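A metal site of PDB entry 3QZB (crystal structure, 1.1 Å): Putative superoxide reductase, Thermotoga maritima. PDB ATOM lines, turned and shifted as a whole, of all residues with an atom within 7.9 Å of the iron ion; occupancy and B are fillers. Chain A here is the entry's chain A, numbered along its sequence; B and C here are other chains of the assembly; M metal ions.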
ATOM      1  N   GLU A  27       5.480 -14.655 -12.730  1.00  0.00           N
ATOM      2  CA  GLU A  27       6.675 -15.176 -13.393  1.00  0.00           C
ATOM      3  C   GLU A  27       6.366 -15.457 -14.863  1.00  0.00           C
ATOM      4  O   GLU A  27       5.582 -16.368 -15.192  1.00  0.00           O
ATOM      5  CB  GLU A  27       7.159 -16.431 -12.678  1.00  0.00           C
ATOM      6  CG  GLU A  27       8.322 -17.156 -13.377  1.00  0.00           C
ATOM      7  CD  GLU A  27       9.518 -16.270 -13.693  1.00  0.00           C
ATOM      8  OE1 GLU A  27      10.197 -15.851 -12.698  1.00  0.00           O
ATOM      9  OE2 GLU A  27       9.744 -16.019 -14.874  1.00  0.00           O
ATOM     10  N   LYS A  28       6.981 -14.680 -15.779  1.00  0.00           N
ATOM     11  CA  LYS A  28       6.753 -14.793 -17.195  1.00  0.00           C
ATOM     12  C   LYS A  28       7.092 -16.179 -17.755  1.00  0.00           C
ATOM     13  O   LYS A  28       6.547 -16.548 -18.794  1.00  0.00           O
ATOM     14  CB  LYS A  28       7.575 -13.750 -17.939  1.00  0.00           C
ATOM     15  CG  LYS A  28       9.069 -13.896 -17.849  1.00  0.00           C
ATOM     16  CD  LYS A  28       9.879 -12.878 -18.615  1.00  0.00           C
ATOM     17  CE  LYS A  28       9.731 -11.482 -18.222  1.00  0.00           C
ATOM     18  NZ  LYS A  28      10.295 -11.337 -16.857  1.00  0.00           N
ATOM     19  N   HIS A  29       8.008 -16.922 -17.146  1.00  0.00           N
ATOM     20  CA  HIS A  29       8.452 -18.156 -17.724  1.00  0.00           C
ATOM     21  C   HIS A  29       7.511 -19.342 -17.543  1.00  0.00           C
ATOM     22  O   HIS A  29       7.724 -20.385 -18.172  1.00  0.00           O
ATOM     23  CB  HIS A  29       9.816 -18.543 -17.162  1.00  0.00           C
ATOM     24  CG  HIS A  29      10.944 -17.700 -17.643  1.00  0.00           C
ATOM     25  ND1 HIS A  29      11.466 -16.651 -16.919  1.00  0.00           N
ATOM     26  CD2 HIS A  29      11.591 -17.730 -18.815  1.00  0.00           C
ATOM     27  CE1 HIS A  29      12.444 -16.117 -17.654  1.00  0.00           C
ATOM     28  NE2 HIS A  29      12.514 -16.727 -18.818  1.00  0.00           N
ATOM     29  N   VAL A  51       3.748 -19.713 -22.998  1.00  0.00           N
ATOM     30  CA  VAL A  51       4.706 -19.033 -22.070  1.00  0.00           C
ATOM     31  C   VAL A  51       4.540 -17.520 -22.350  1.00  0.00           C
ATOM     32  O   VAL A  51       4.431 -17.090 -23.475  1.00  0.00           O
ATOM     33  CB  VAL A  51       6.142 -19.501 -22.324  1.00  0.00           C
ATOM     34  CG1 VAL A  51       7.144 -18.727 -21.458  1.00  0.00           C
ATOM     35  CG2 VAL A  51       6.264 -21.016 -22.045  1.00  0.00           C
ATOM     36  N   HIS A  57       7.114 -12.460 -22.361  1.00  0.00           N
ATOM     37  CA  HIS A  57       8.496 -12.884 -22.423  1.00  0.00           C
ATOM     38  C   HIS A  57       9.092 -12.367 -23.729  1.00  0.00           C
ATOM     39  O   HIS A  57       8.457 -12.415 -24.768  1.00  0.00           O
ATOM     40  CB  HIS A  57       8.622 -14.430 -22.336  1.00  0.00           C
ATOM     41  CG  HIS A  57      10.046 -14.912 -22.201  1.00  0.00           C
ATOM     42  ND1 HIS A  57      10.910 -14.952 -23.279  1.00  0.00           N
ATOM     43  CD2 HIS A  57      10.764 -15.340 -21.133  1.00  0.00           C
ATOM     44  CE1 HIS A  57      12.099 -15.375 -22.884  1.00  0.00           C
ATOM     45  NE2 HIS A  57      12.048 -15.608 -21.587  1.00  0.00           N
ATOM     46  N   PRO A  58      10.372 -11.894 -23.691  1.00  0.00           N
ATOM     47  CA  PRO A  58      11.027 -11.488 -24.933  1.00  0.00           C
ATOM     48  C   PRO A  58      11.089 -12.534 -26.007  1.00  0.00           C
ATOM     49  O   PRO A  58      11.058 -13.766 -25.711  1.00  0.00           O
ATOM     50  CB  PRO A  58      12.442 -11.115 -24.448  1.00  0.00           C
ATOM     51  CG  PRO A  58      12.262 -10.718 -23.031  1.00  0.00           C
ATOM     52  CD  PRO A  58      11.207 -11.665 -22.506  1.00  0.00           C
ATOM     53  N   HIS A  63      17.539 -13.795 -26.667  1.00  0.00           N
ATOM     54  CA  HIS A  63      16.753 -14.264 -25.522  1.00  0.00           C
ATOM     55  C   HIS A  63      15.365 -14.649 -26.027  1.00  0.00           C
ATOM     56  O   HIS A  63      14.581 -13.797 -26.425  1.00  0.00           O
ATOM     57  CB  HIS A  63      16.632 -13.178 -24.457  1.00  0.00           C
ATOM     58  CG  HIS A  63      15.857 -13.580 -23.247  1.00  0.00           C
ATOM     59  ND1 HIS A  63      15.257 -12.655 -22.443  1.00  0.00           N
ATOM     60  CD2 HIS A  63      15.531 -14.809 -22.736  1.00  0.00           C
ATOM     61  CE1 HIS A  63      14.611 -13.289 -21.467  1.00  0.00           C
ATOM     62  NE2 HIS A  63      14.762 -14.616 -21.625  1.00  0.00           N
ATOM     63  N   HIS A  64      15.012 -15.925 -25.881  1.00  0.00           N
ATOM     64  CA  HIS A  64      13.747 -16.424 -26.392  1.00  0.00           C
ATOM     65  C   HIS A  64      13.412 -17.767 -25.789  1.00  0.00           C
ATOM     66  O   HIS A  64      14.291 -18.512 -25.352  1.00  0.00           O
ATOM     67  CB  HIS A  64      13.812 -16.546 -27.933  1.00  0.00           C
ATOM     68  CG  HIS A  64      15.008 -17.347 -28.425  1.00  0.00           C
ATOM     69  ND1 HIS A  64      16.127 -16.732 -28.932  1.00  0.00           N
ATOM     70  CD2 HIS A  64      15.263 -18.667 -28.461  1.00  0.00           C
ATOM     71  CE1 HIS A  64      17.004 -17.671 -29.260  1.00  0.00           C
ATOM     72  NE2 HIS A  64      16.533 -18.849 -28.949  1.00  0.00           N
ATOM     73  N   ILE A  65      12.124 -18.072 -25.796  1.00  0.00           N
ATOM     74  CA  ILE A  65      11.661 -19.443 -25.468  1.00  0.00           C
ATOM     75  C   ILE A  65      11.866 -20.349 -26.659  1.00  0.00           C
ATOM     76  O   ILE A  65      11.451 -20.074 -27.762  1.00  0.00           O
ATOM     77  CB  ILE A  65      10.180 -19.397 -25.083  1.00  0.00           C
ATOM     78  CG1 ILE A  65       9.911 -18.414 -23.928  1.00  0.00           C
ATOM     79  CG2 ILE A  65       9.665 -20.830 -24.781  1.00  0.00           C
ATOM     80  CD1 ILE A  65      10.722 -18.699 -22.689  1.00  0.00           C
ATOM     81  N   TYR A 126      11.343 -24.350 -22.043  1.00  0.00           N
ATOM     82  CA  TYR A 126      12.768 -24.060 -21.984  1.00  0.00           C
ATOM     83  C   TYR A 126      13.032 -22.703 -22.617  1.00  0.00           C
ATOM     84  O   TYR A 126      12.699 -22.464 -23.771  1.00  0.00           O
ATOM     85  CB  TYR A 126      13.554 -25.154 -22.756  1.00  0.00           C
ATOM     86  CG  TYR A 126      15.044 -24.935 -22.751  1.00  0.00           C
ATOM     87  CD1 TYR A 126      15.767 -24.941 -21.564  1.00  0.00           C
ATOM     88  CD2 TYR A 126      15.700 -24.670 -23.903  1.00  0.00           C
ATOM     89  CE1 TYR A 126      17.136 -24.651 -21.577  1.00  0.00           C
ATOM     90  CE2 TYR A 126      17.078 -24.383 -23.936  1.00  0.00           C
ATOM     91  CZ  TYR A 126      17.755 -24.366 -22.758  1.00  0.00           C
ATOM     92  OH  TYR A 126      19.109 -24.039 -22.729  1.00  0.00           O
ATOM     93  N   CYS A 127      13.699 -21.839 -21.823  1.00  0.00           N
ATOM     94  CA  CYS A 127      14.233 -20.548 -22.275  1.00  0.00           C
ATOM     95  C   CYS A 127      15.692 -20.736 -22.559  1.00  0.00           C
ATOM     96  O   CYS A 127      16.393 -21.490 -21.896  1.00  0.00           O
ATOM     97  CB  CYS A 127      14.001 -19.535 -21.157  1.00  0.00           C
ATOM     98  SG  CYS A 127      14.784 -17.931 -21.592  1.00  0.00           S
ATOM     99  N   ASN A 128      16.172 -20.073 -23.597  1.00  0.00           N
ATOM    100  CA  ASN A 128      17.592 -20.223 -23.990  1.00  0.00           C
ATOM    101  C   ASN A 128      18.577 -19.699 -22.932  1.00  0.00           C
ATOM    102  O   ASN A 128      19.739 -20.121 -22.958  1.00  0.00           O
ATOM    103  CB  ASN A 128      17.889 -19.635 -25.357  1.00  0.00           C
ATOM    104  CG  ASN A 128      17.945 -18.127 -25.373  1.00  0.00           C
ATOM    105  OD1 ASN A 128      17.242 -17.461 -24.609  1.00  0.00           O
ATOM    106  ND2 ASN A 128      18.751 -17.575 -26.281  1.00  0.00           N
ATOM    107  N   ILE A 129      18.127 -18.859 -21.971  1.00  0.00           N
ATOM    108  CA  ILE A 129      19.014 -18.399 -20.919  1.00  0.00           C
ATOM    109  C   ILE A 129      18.460 -18.577 -19.518  1.00  0.00           C
ATOM    110  O   ILE A 129      19.198 -18.427 -18.561  1.00  0.00           O
ATOM    111  CB  ILE A 129      19.442 -16.896 -21.148  1.00  0.00           C
ATOM    112  CG1 ILE A 129      18.268 -15.949 -20.946  1.00  0.00           C
ATOM    113  CG2 ILE A 129      20.112 -16.757 -22.488  1.00  0.00           C
ATOM    114  CD1 ILE A 129      18.603 -14.477 -21.209  1.00  0.00           C
ATOM    115  N   HIS A 130      17.165 -18.925 -19.348  1.00  0.00           N
ATOM    116  CA  HIS A 130      16.567 -19.075 -18.036  1.00  0.00           C
ATOM    117  C   HIS A 130      16.079 -20.498 -17.743  1.00  0.00           C
ATOM    118  O   HIS A 130      15.266 -20.715 -16.822  1.00  0.00           O
ATOM    119  CB  HIS A 130      15.397 -18.096 -17.842  1.00  0.00           C
ATOM    120  CG  HIS A 130      15.817 -16.659 -17.895  1.00  0.00           C
ATOM    121  ND1 HIS A 130      15.317 -15.756 -18.836  1.00  0.00           N
ATOM    122  CD2 HIS A 130      16.666 -15.951 -17.088  1.00  0.00           C
ATOM    123  CE1 HIS A 130      15.860 -14.580 -18.583  1.00  0.00           C
ATOM    124  NE2 HIS A 130      16.668 -14.658 -17.560  1.00  0.00           N
ATOM    125  N   GLY A 131      16.611 -21.474 -18.481  1.00  0.00           N
ATOM    126  CA  GLY A 131      16.381 -22.868 -18.151  1.00  0.00           C
ATOM    127  C   GLY A 131      14.950 -23.353 -18.243  1.00  0.00           C
ATOM    128  O   GLY A 131      14.169 -22.901 -19.089  1.00  0.00           O
ATOM    129  N   TRP A 133      11.128 -24.892 -16.931  1.00  0.00           N
ATOM    130  CA  TRP A 133       9.964 -24.494 -16.175  1.00  0.00           C
ATOM    131  C   TRP A 133       8.868 -25.504 -16.437  1.00  0.00           C
ATOM    132  O   TRP A 133       8.752 -26.041 -17.539  1.00  0.00           O
ATOM    133  CB  TRP A 133       9.486 -23.092 -16.669  1.00  0.00           C
ATOM    134  CG  TRP A 133      10.544 -22.070 -16.468  1.00  0.00           C
ATOM    135  CD1 TRP A 133      11.648 -21.871 -17.254  1.00  0.00           C
ATOM    136  CD2 TRP A 133      10.707 -21.202 -15.342  1.00  0.00           C
ATOM    137  NE1 TRP A 133      12.444 -20.894 -16.700  1.00  0.00           N
ATOM    138  CE2 TRP A 133      11.907 -20.519 -15.512  1.00  0.00           C
ATOM    139  CE3 TRP A 133       9.945 -20.971 -14.198  1.00  0.00           C
ATOM    140  CZ2 TRP A 133      12.346 -19.534 -14.593  1.00  0.00           C
ATOM    141  CZ3 TRP A 133      10.376 -20.026 -13.293  1.00  0.00           C
ATOM    142  CH2 TRP A 133      11.567 -19.338 -13.472  1.00  0.00           C
ATOM    143  N   VAL B  95      22.388 -15.093 -19.471  1.00  0.00           N
ATOM    144  CA  VAL B  95      21.826 -13.874 -18.827  1.00  0.00           C
ATOM    145  C   VAL B  95      22.886 -12.746 -18.849  1.00  0.00           C
ATOM    146  O   VAL B  95      22.559 -11.552 -18.893  1.00  0.00           O
ATOM    147  CB  VAL B  95      21.385 -14.209 -17.385  1.00  0.00           C
ATOM    148  CG1 VAL B  95      21.207 -12.962 -16.471  1.00  0.00           C
ATOM    149  CG2 VAL B  95      20.039 -14.937 -17.452  1.00  0.00           C
ATOM    150  N   TYR C  79      20.783 -22.269 -13.701  1.00  0.00           N
ATOM    151  CA  TYR C  79      20.024 -22.900 -14.772  1.00  0.00           C
ATOM    152  C   TYR C  79      20.745 -24.134 -15.344  1.00  0.00           C
ATOM    153  O   TYR C  79      21.943 -24.323 -15.162  1.00  0.00           O
ATOM    154  CB  TYR C  79      19.744 -21.878 -15.880  1.00  0.00           C
ATOM    155  CG  TYR C  79      19.095 -20.607 -15.365  1.00  0.00           C
ATOM    156  CD1 TYR C  79      17.826 -20.634 -14.780  1.00  0.00           C
ATOM    157  CD2 TYR C  79      19.734 -19.408 -15.420  1.00  0.00           C
ATOM    158  CE1 TYR C  79      17.233 -19.498 -14.303  1.00  0.00           C
ATOM    159  CE2 TYR C  79      19.176 -18.246 -14.920  1.00  0.00           C
ATOM    160  CZ  TYR C  79      17.926 -18.305 -14.327  1.00  0.00           C
ATOM    161  OH  TYR C  79      17.328 -17.156 -13.839  1.00  0.00           O
HETATM  162 FE    FE M   1      13.867 -16.150 -20.405  1.00  0.00          FE
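A ring nitrogen (ND1) of His 29 lies within hydrogen-bond range of the side-chain carboxylate (OE2) of Glu 27. The backbone carbonyl oxygen (O) of His 130 lies within hydrogen-bond range of the indole nitrogen (NE1) of Trp 133 (2.8 Å). SG of Cys 127 sits close to N of Ile 129 (3.5 Å).
Five residues have an atom within 4 Å of the iron ion: His 29, His 57, His 63, Cys 127 and His 130. The nearest printed residue that does not touch the iron ion is Ile 129 (4.4 Å).
The iron ion is bound by a ring nitrogen (NE2) of His 63, a ring nitrogen (NE2) of His 29, a ring nitrogen (ND1) of His 130, a ring nitrogen (NE2) of His 57 and the side-chain sulfur of Cys 127. The iron ion has five donor atoms within binding distance.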
